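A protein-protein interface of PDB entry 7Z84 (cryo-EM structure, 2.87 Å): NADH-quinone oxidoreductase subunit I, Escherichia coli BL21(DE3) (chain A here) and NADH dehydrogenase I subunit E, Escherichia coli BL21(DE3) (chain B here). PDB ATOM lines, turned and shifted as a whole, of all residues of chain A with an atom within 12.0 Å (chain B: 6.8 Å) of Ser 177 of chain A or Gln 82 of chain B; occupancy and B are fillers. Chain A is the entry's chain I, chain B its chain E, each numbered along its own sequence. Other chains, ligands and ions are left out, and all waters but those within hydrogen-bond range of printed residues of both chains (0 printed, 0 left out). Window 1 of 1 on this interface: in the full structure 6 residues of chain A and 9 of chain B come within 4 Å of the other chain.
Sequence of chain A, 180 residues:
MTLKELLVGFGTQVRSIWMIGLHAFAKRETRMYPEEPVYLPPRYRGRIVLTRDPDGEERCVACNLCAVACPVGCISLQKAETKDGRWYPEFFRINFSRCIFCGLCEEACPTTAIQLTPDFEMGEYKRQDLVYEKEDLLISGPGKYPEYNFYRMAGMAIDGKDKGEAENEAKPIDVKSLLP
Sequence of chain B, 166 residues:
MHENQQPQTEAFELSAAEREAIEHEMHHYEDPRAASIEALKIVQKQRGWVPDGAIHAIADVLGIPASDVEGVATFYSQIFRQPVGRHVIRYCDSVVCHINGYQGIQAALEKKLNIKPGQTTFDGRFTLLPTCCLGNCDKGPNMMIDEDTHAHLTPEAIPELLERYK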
ATOM      1  N   LYS A 171       5.909 -17.888 -17.827  1.00  0.00           N
ATOM      2  CA  LYS A 171       5.756 -18.148 -16.406  1.00  0.00           C
ATOM      3  C   LYS A 171       6.065 -16.883 -15.604  1.00  0.00           C
ATOM      4  O   LYS A 171       6.919 -16.084 -15.997  1.00  0.00           O
ATOM      5  CB  LYS A 171       6.675 -19.284 -15.968  1.00  0.00           C
ATOM      6  CG  LYS A 171       5.950 -20.583 -15.664  1.00  0.00           C
ATOM      7  CD  LYS A 171       6.894 -21.771 -15.736  1.00  0.00           C
ATOM      8  CE  LYS A 171       7.179 -22.170 -17.172  1.00  0.00           C
ATOM      9  NZ  LYS A 171       6.046 -22.929 -17.767  1.00  0.00           N
ATOM     10  N   PRO A 172       5.364 -16.664 -14.491  1.00  0.00           N
ATOM     11  CA  PRO A 172       5.615 -15.458 -13.694  1.00  0.00           C
ATOM     12  C   PRO A 172       6.972 -15.509 -13.012  1.00  0.00           C
ATOM     13  O   PRO A 172       7.354 -16.515 -12.412  1.00  0.00           O
ATOM     14  CB  PRO A 172       4.473 -15.461 -12.671  1.00  0.00           C
ATOM     15  CG  PRO A 172       4.018 -16.870 -12.607  1.00  0.00           C
ATOM     16  CD  PRO A 172       4.229 -17.444 -13.971  1.00  0.00           C
ATOM     17  N   ILE A 173       7.700 -14.402 -13.114  1.00  0.00           N
ATOM     18  CA  ILE A 173       9.018 -14.261 -12.511  1.00  0.00           C
ATOM     19  C   ILE A 173       8.864 -13.447 -11.237  1.00  0.00           C
ATOM     20  O   ILE A 173       8.339 -12.328 -11.265  1.00  0.00           O
ATOM     21  CB  ILE A 173      10.009 -13.597 -13.477  1.00  0.00           C
ATOM     22  CG1 ILE A 173      10.120 -14.406 -14.769  1.00  0.00           C
ATOM     23  CG2 ILE A 173      11.369 -13.440 -12.822  1.00  0.00           C
ATOM     24  CD1 ILE A 173      10.693 -13.626 -15.926  1.00  0.00           C
ATOM     25  N   ASP A 174       9.310 -14.010 -10.120  1.00  0.00           N
ATOM     26  CA  ASP A 174       9.244 -13.306  -8.849  1.00  0.00           C
ATOM     27  C   ASP A 174      10.255 -12.166  -8.815  1.00  0.00           C
ATOM     28  O   ASP A 174      11.311 -12.221  -9.448  1.00  0.00           O
ATOM     29  CB  ASP A 174       9.503 -14.270  -7.694  1.00  0.00           C
ATOM     30  CG  ASP A 174       8.676 -13.944  -6.468  1.00  0.00           C
ATOM     31  OD1 ASP A 174       9.225 -13.995  -5.349  1.00  0.00           O
ATOM     32  OD2 ASP A 174       7.477 -13.637  -6.624  1.00  0.00           O
ATOM     33  N   VAL A 175       9.914 -11.117  -8.062  1.00  0.00           N
ATOM     34  CA  VAL A 175      10.837 -10.003  -7.883  1.00  0.00           C
ATOM     35  C   VAL A 175      11.990 -10.378  -6.963  1.00  0.00           C
ATOM     36  O   VAL A 175      13.005  -9.674  -6.926  1.00  0.00           O
ATOM     37  CB  VAL A 175      10.090  -8.769  -7.345  1.00  0.00           C
ATOM     38  CG1 VAL A 175       9.182  -8.198  -8.417  1.00  0.00           C
ATOM     39  CG2 VAL A 175       9.291  -9.130  -6.106  1.00  0.00           C
ATOM     40  N   LYS A 176      11.860 -11.475  -6.223  1.00  0.00           N
ATOM     41  CA  LYS A 176      12.902 -11.974  -5.339  1.00  0.00           C
ATOM     42  C   LYS A 176      13.849 -12.944  -6.034  1.00  0.00           C
ATOM     43  O   LYS A 176      14.706 -13.533  -5.369  1.00  0.00           O
ATOM     44  CB  LYS A 176      12.270 -12.652  -4.121  1.00  0.00           C
ATOM     45  CG  LYS A 176      11.098 -11.892  -3.527  1.00  0.00           C
ATOM     46  CD  LYS A 176      11.090 -11.982  -2.014  1.00  0.00           C
ATOM     47  CE  LYS A 176      10.524 -13.310  -1.547  1.00  0.00           C
ATOM     48  NZ  LYS A 176       9.256 -13.646  -2.250  1.00  0.00           N
ATOM     49  N   SER A 177      13.704 -13.132  -7.342  1.00  0.00           N
ATOM     50  CA  SER A 177      14.558 -14.056  -8.075  1.00  0.00           C
ATOM     51  C   SER A 177      15.989 -13.534  -8.150  1.00  0.00           C
ATOM     52  O   SER A 177      16.237 -12.326  -8.163  1.00  0.00           O
ATOM     53  CB  SER A 177      14.013 -14.284  -9.484  1.00  0.00           C
ATOM     54  OG  SER A 177      14.206 -13.139 -10.294  1.00  0.00           O
ATOM     55  N   LEU A 178      16.937 -14.470  -8.200  1.00  0.00           N
ATOM     56  CA  LEU A 178      18.352 -14.122  -8.194  1.00  0.00           C
ATOM     57  C   LEU A 178      18.854 -13.644  -9.547  1.00  0.00           C
ATOM     58  O   LEU A 178      19.917 -13.016  -9.609  1.00  0.00           O
ATOM     59  CB  LEU A 178      19.181 -15.323  -7.740  1.00  0.00           C
ATOM     60  CG  LEU A 178      18.662 -16.073  -6.515  1.00  0.00           C
ATOM     61  CD1 LEU A 178      19.383 -17.399  -6.365  1.00  0.00           C
ATOM     62  CD2 LEU A 178      18.825 -15.224  -5.268  1.00  0.00           C
ATOM     63  N   LEU A 179      18.132 -13.934 -10.624  1.00  0.00           N
ATOM     64  CA  LEU A 179      18.584 -13.540 -11.949  1.00  0.00           C
ATOM     65  C   LEU A 179      18.427 -12.031 -12.132  1.00  0.00           C
ATOM     66  O   LEU A 179      17.445 -11.448 -11.663  1.00  0.00           O
ATOM     67  CB  LEU A 179      17.795 -14.284 -13.026  1.00  0.00           C
ATOM     68  CG  LEU A 179      18.070 -15.784 -13.140  1.00  0.00           C
ATOM     69  CD1 LEU A 179      16.992 -16.467 -13.964  1.00  0.00           C
ATOM     70  CD2 LEU A 179      19.441 -16.033 -13.739  1.00  0.00           C
ATOM     71  N   PRO A 180      19.382 -11.368 -12.802  1.00  0.00           N
ATOM     72  CA  PRO A 180      19.314  -9.922 -13.043  1.00  0.00           C
ATOM     73  C   PRO A 180      18.173  -9.523 -13.978  1.00  0.00           C
ATOM     74  O   PRO A 180      17.636 -10.380 -14.680  1.00  0.00           O
ATOM     75  CB  PRO A 180      20.671  -9.605 -13.685  1.00  0.00           C
ATOM     76  CG  PRO A 180      21.549 -10.757 -13.336  1.00  0.00           C
ATOM     77  CD  PRO A 180      20.645 -11.943 -13.293  1.00  0.00           C
ATOM     78  N   GLN B  44      23.047  -9.658   4.529  1.00  0.00           N
ATOM     79  CA  GLN B  44      23.437 -10.631   3.513  1.00  0.00           C
ATOM     80  C   GLN B  44      24.815 -11.219   3.794  1.00  0.00           C
ATOM     81  O   GLN B  44      25.030 -12.419   3.606  1.00  0.00           O
ATOM     82  CB  GLN B  44      23.402  -9.969   2.135  1.00  0.00           C
ATOM     83  CG  GLN B  44      23.924 -10.827   1.001  1.00  0.00           C
ATOM     84  CD  GLN B  44      23.285 -10.478  -0.323  1.00  0.00           C
ATOM     85  OE1 GLN B  44      22.086 -10.672  -0.517  1.00  0.00           O
ATOM     86  NE2 GLN B  44      24.084  -9.956  -1.245  1.00  0.00           N
ATOM     87  N   GLY B  48      24.226 -14.913   4.341  1.00  0.00           N
ATOM     88  CA  GLY B  48      24.198 -15.416   2.984  1.00  0.00           C
ATOM     89  C   GLY B  48      23.162 -14.763   2.091  1.00  0.00           C
ATOM     90  O   GLY B  48      23.418 -14.567   0.898  1.00  0.00           O
ATOM     91  N   TRP B  49      22.001 -14.420   2.640  1.00  0.00           N
ATOM     92  CA  TRP B  49      20.930 -13.784   1.888  1.00  0.00           C
ATOM     93  C   TRP B  49      20.096 -12.951   2.854  1.00  0.00           C
ATOM     94  O   TRP B  49      20.393 -12.868   4.049  1.00  0.00           O
ATOM     95  CB  TRP B  49      20.075 -14.822   1.154  1.00  0.00           C
ATOM     96  CG  TRP B  49      19.250 -15.690   2.059  1.00  0.00           C
ATOM     97  CD1 TRP B  49      19.708 -16.537   3.026  1.00  0.00           C
ATOM     98  CD2 TRP B  49      17.822 -15.795   2.081  1.00  0.00           C
ATOM     99  NE1 TRP B  49      18.656 -17.161   3.647  1.00  0.00           N
ATOM    100  CE2 TRP B  49      17.487 -16.723   3.085  1.00  0.00           C
ATOM    101  CE3 TRP B  49      16.796 -15.194   1.348  1.00  0.00           C
ATOM    102  CZ2 TRP B  49      16.169 -17.064   3.374  1.00  0.00           C
ATOM    103  CZ3 TRP B  49      15.489 -15.534   1.637  1.00  0.00           C
ATOM    104  CH2 TRP B  49      15.186 -16.460   2.639  1.00  0.00           C
ATOM    105  N   VAL B  50      19.047 -12.330   2.327  1.00  0.00           N
ATOM    106  CA  VAL B  50      18.173 -11.480   3.131  1.00  0.00           C
ATOM    107  C   VAL B  50      16.819 -12.162   3.294  1.00  0.00           C
ATOM    108  O   VAL B  50      16.022 -12.186   2.346  1.00  0.00           O
ATOM    109  CB  VAL B  50      18.017 -10.087   2.502  1.00  0.00           C
ATOM    110  CG1 VAL B  50      17.186  -9.195   3.400  1.00  0.00           C
ATOM    111  CG2 VAL B  50      19.377  -9.467   2.243  1.00  0.00           C
ATOM    112  N   THR B  74      14.607  -5.838  -3.670  1.00  0.00           N
ATOM    113  CA  THR B  74      14.246  -6.439  -4.946  1.00  0.00           C
ATOM    114  C   THR B  74      14.774  -5.657  -6.142  1.00  0.00           C
ATOM    115  O   THR B  74      14.828  -6.208  -7.246  1.00  0.00           O
ATOM    116  CB  THR B  74      12.729  -6.568  -5.055  1.00  0.00           C
ATOM    117  OG1 THR B  74      12.121  -5.337  -4.653  1.00  0.00           O
ATOM    118  CG2 THR B  74      12.226  -7.688  -4.164  1.00  0.00           C
ATOM    119  N   TYR B  76      17.959  -4.252  -6.403  1.00  0.00           N
ATOM    120  CA  TYR B  76      19.383  -4.460  -6.619  1.00  0.00           C
ATOM    121  C   TYR B  76      19.673  -5.943  -6.800  1.00  0.00           C
ATOM    122  O   TYR B  76      19.188  -6.778  -6.031  1.00  0.00           O
ATOM    123  CB  TYR B  76      20.183  -3.887  -5.450  1.00  0.00           C
ATOM    124  CG  TYR B  76      20.128  -2.379  -5.389  1.00  0.00           C
ATOM    125  CD1 TYR B  76      20.904  -1.600  -6.232  1.00  0.00           C
ATOM    126  CD2 TYR B  76      19.283  -1.735  -4.500  1.00  0.00           C
ATOM    127  CE1 TYR B  76      20.843  -0.222  -6.179  1.00  0.00           C
ATOM    128  CE2 TYR B  76      19.213  -0.364  -4.445  1.00  0.00           C
ATOM    129  CZ  TYR B  76      19.994   0.388  -5.286  1.00  0.00           C
ATOM    130  OH  TYR B  76      19.922   1.756  -5.225  1.00  0.00           O
ATOM    131  N   SER B  77      20.466  -6.262  -7.826  1.00  0.00           N
ATOM    132  CA  SER B  77      20.702  -7.657  -8.178  1.00  0.00           C
ATOM    133  C   SER B  77      21.621  -8.354  -7.183  1.00  0.00           C
ATOM    134  O   SER B  77      21.525  -9.573  -7.010  1.00  0.00           O
ATOM    135  CB  SER B  77      21.283  -7.744  -9.588  1.00  0.00           C
ATOM    136  OG  SER B  77      22.458  -6.964  -9.703  1.00  0.00           O
ATOM    137  N   ILE B  79      21.655  -7.957  -3.949  1.00  0.00           N
ATOM    138  CA  ILE B  79      20.953  -8.244  -2.705  1.00  0.00           C
ATOM    139  C   ILE B  79      20.006  -9.398  -2.992  1.00  0.00           C
ATOM    140  O   ILE B  79      19.046  -9.252  -3.758  1.00  0.00           O
ATOM    141  CB  ILE B  79      20.202  -7.018  -2.172  1.00  0.00           C
ATOM    142  CG1 ILE B  79      21.187  -5.922  -1.767  1.00  0.00           C
ATOM    143  CG2 ILE B  79      19.329  -7.405  -0.990  1.00  0.00           C
ATOM    144  CD1 ILE B  79      20.546  -4.566  -1.599  1.00  0.00           C
ATOM    145  N   PHE B  80      20.270 -10.548  -2.383  1.00  0.00           N
ATOM    146  CA  PHE B  80      19.545 -11.771  -2.692  1.00  0.00           C
ATOM    147  C   PHE B  80      18.391 -11.939  -1.712  1.00  0.00           C
ATOM    148  O   PHE B  80      18.606 -12.010  -0.497  1.00  0.00           O
ATOM    149  CB  PHE B  80      20.482 -12.975  -2.641  1.00  0.00           C
ATOM    150  CG  PHE B  80      21.720 -12.813  -3.474  1.00  0.00           C
ATOM    151  CD1 PHE B  80      21.640 -12.336  -4.772  1.00  0.00           C
ATOM    152  CD2 PHE B  80      22.965 -13.128  -2.958  1.00  0.00           C
ATOM    153  CE1 PHE B  80      22.777 -12.180  -5.540  1.00  0.00           C
ATOM    154  CE2 PHE B  80      24.107 -12.977  -3.722  1.00  0.00           C
ATOM    155  CZ  PHE B  80      24.012 -12.501  -5.014  1.00  0.00           C
ATOM    156  N   ARG B  81      17.172 -11.998  -2.242  1.00  0.00           N
ATOM    157  CA  ARG B  81      15.978 -12.226  -1.444  1.00  0.00           C
ATOM    158  C   ARG B  81      15.511 -13.674  -1.508  1.00  0.00           C
ATOM    159  O   ARG B  81      14.431 -13.991  -1.000  1.00  0.00           O
ATOM    160  CB  ARG B  81      14.860 -11.286  -1.892  1.00  0.00           C
ATOM    161  CG  ARG B  81      14.970  -9.887  -1.318  1.00  0.00           C
ATOM    162  CD  ARG B  81      14.815  -9.905   0.188  1.00  0.00           C
ATOM    163  NE  ARG B  81      13.414  -9.870   0.586  1.00  0.00           N
ATOM    164  CZ  ARG B  81      12.769 -10.884   1.143  1.00  0.00           C
ATOM    165  NH1 ARG B  81      13.369 -12.037   1.386  1.00  0.00           N
ATOM    166  NH2 ARG B  81      11.486 -10.739   1.465  1.00  0.00           N
ATOM    167  N   GLN B  82      16.297 -14.549  -2.122  1.00  0.00           N
ATOM    168  CA  GLN B  82      16.072 -15.983  -2.159  1.00  0.00           C
ATOM    169  C   GLN B  82      17.334 -16.686  -1.684  1.00  0.00           C
ATOM    170  O   GLN B  82      18.439 -16.167  -1.872  1.00  0.00           O
ATOM    171  CB  GLN B  82      15.709 -16.452  -3.576  1.00  0.00           C
ATOM    172  CG  GLN B  82      14.248 -16.834  -3.738  1.00  0.00           C
ATOM    173  CD  GLN B  82      13.764 -16.698  -5.164  1.00  0.00           C
ATOM    174  OE1 GLN B  82      14.515 -16.922  -6.112  1.00  0.00           O
ATOM    175  NE2 GLN B  82      12.499 -16.330  -5.327  1.00  0.00           N
ATOM    176  N   PRO B  83      17.204 -17.849  -1.039  1.00  0.00           N
ATOM    177  CA  PRO B  83      18.389 -18.517  -0.482  1.00  0.00           C
ATOM    178  C   PRO B  83      19.338 -19.011  -1.564  1.00  0.00           C
ATOM    179  O   PRO B  83      18.917 -19.534  -2.598  1.00  0.00           O
ATOM    180  CB  PRO B  83      17.798 -19.685   0.316  1.00  0.00           C
ATOM    181  CG  PRO B  83      16.453 -19.909  -0.276  1.00  0.00           C
ATOM    182  CD  PRO B  83      15.963 -18.555  -0.676  1.00  0.00           C
ATOM    183  N   VAL B  84      20.632 -18.837  -1.308  1.00  0.00           N
ATOM    184  CA  VAL B  84      21.686 -19.223  -2.233  1.00  0.00           C
ATOM    185  C   VAL B  84      22.574 -20.259  -1.553  1.00  0.00           C
ATOM    186  O   VAL B  84      22.410 -20.577  -0.376  1.00  0.00           O
ATOM    187  CB  VAL B  84      22.521 -18.018  -2.707  1.00  0.00           C
ATOM    188  CG1 VAL B  84      21.638 -16.993  -3.395  1.00  0.00           C
ATOM    189  CG2 VAL B  84      23.257 -17.392  -1.535  1.00  0.00           C
ATOM    190  N   GLY B 118      21.090 -19.334 -12.278  1.00  0.00           N
ATOM    191  CA  GLY B 118      20.035 -18.944 -11.372  1.00  0.00           C
ATOM    192  C   GLY B 118      19.600 -20.019 -10.402  1.00  0.00           C
ATOM    193  O   GLY B 118      18.732 -19.755  -9.560  1.00  0.00           O
ATOM    194  N   LEU B 129      25.231 -17.898 -11.332  1.00  0.00           N
ATOM    195  CA  LEU B 129      24.525 -16.688 -11.693  1.00  0.00           C
ATOM    196  C   LEU B 129      25.263 -15.957 -12.808  1.00  0.00           C
ATOM    197  O   LEU B 129      26.501 -15.806 -12.741  1.00  0.00           O
ATOM    198  CB  LEU B 129      24.369 -15.768 -10.478  1.00  0.00           C
ATOM    199  CG  LEU B 129      23.200 -16.043  -9.533  1.00  0.00           C
ATOM    200  CD1 LEU B 129      23.303 -15.178  -8.290  1.00  0.00           C
ATOM    201  CD2 LEU B 129      21.886 -15.806 -10.247  1.00  0.00           C
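OE1 of Gln 82 of chain B sits close to O of Lys 176 of chain A (3.5 Å).
The side-chain amide oxygen (OE1) of Gln 44 of chain B lies within hydrogen-bond range of the backbone NH (N) of Phe 80 of chain B (2.6 Å). The backbone carbonyl oxygen (O) of Phe 80 of chain B lies within hydrogen-bond range of the backbone NH (N) of Val 50 of chain B (2.9 Å). The guanidinium group (NH1) of Arg 81 of chain B lies within hydrogen-bond range of the backbone carbonyl oxygen (O) of Val 50 of chain B (2.8 Å). The side-chain amino group (NZ) of Lys 176 of chain A lies within salt-bridge range of the side-chain carboxylate (OD1) of Asp 174 of chain A, at 3.1 Å. The side-chain hydroxyl (OG) of Ser 177 of chain A sits at hydrogen-bond distance from the backbone carbonyl oxygen (O) of Asp 174 of chain A, at 3.2 Å.
Among the printed residues, merely in contact across the chains: Leu 178 of chain A with Leu 129 of chain B (3.5 Å), Ser 177 of chain A with Gln 82 of chain B (3.5 Å), Val 175 of chain A with Thr 74 of chain B (3.5 Å), Leu 178 of chain A with Gln 82 of chain B (3.5 Å), Lys 176 of chain A with Arg 81 of chain B (3.7 Å), Leu 178 of chain A with Val 84 of chain B (3.8 Å), Leu 179 of chain A with Gly 118 of chain B (3.8 Å) and Leu 178 of chain A with Phe 80 of chain B (3.8 Å).
Ser 177 of chain A touches just one residue of chain B: Gln 82 (3.5 Å). Of chain A, only Lys 176 (3.3 Å), Ser 177 (3.5 Å) and Leu 178 (3.5 Å) come within 4 Å of Gln 82 of chain B. Phe 80 of chain B touches just one residue of chain A: Leu 178 (3.8 Å). Arg 81 of chain B touches just one residue of chain A: Lys 176. No residue of chain A comes within 4 Å of Pro 83 of chain B. Val 84 of chain B touches just one residue of chain A: Leu 178. Printed residues of chain A within 4 Å of Thr 74 of chain B: Val 175. Of the printed residues of chain A, Gly 118 of chain B touches Leu 179. Printed residues of chain B within 4 Å of Leu 178 of chain A: Phe 80, Gln 82, Val 84 and Leu 129. Tyr 76 of chain B touches none of the printed residues of chain A. Pro 180 of chain A touches none of the printed residues of chain B. The nearest residue of chain B that does not touch Ser 177 of chain A is Arg 81 of chain B (5.9 Å). The nearest residue of chain A that does not touch Gln 82 of chain B is Asp 174 of chain A (4.02 Å). The nearest printed residue of chain A that does not touch Thr 74 of chain B is Lys 176 of chain A (4.3 Å).
Of the 10 printed residues of chain A, 5 touch a printed residue of chain B. Among the printed residues, 9 pairs touch across the chains.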
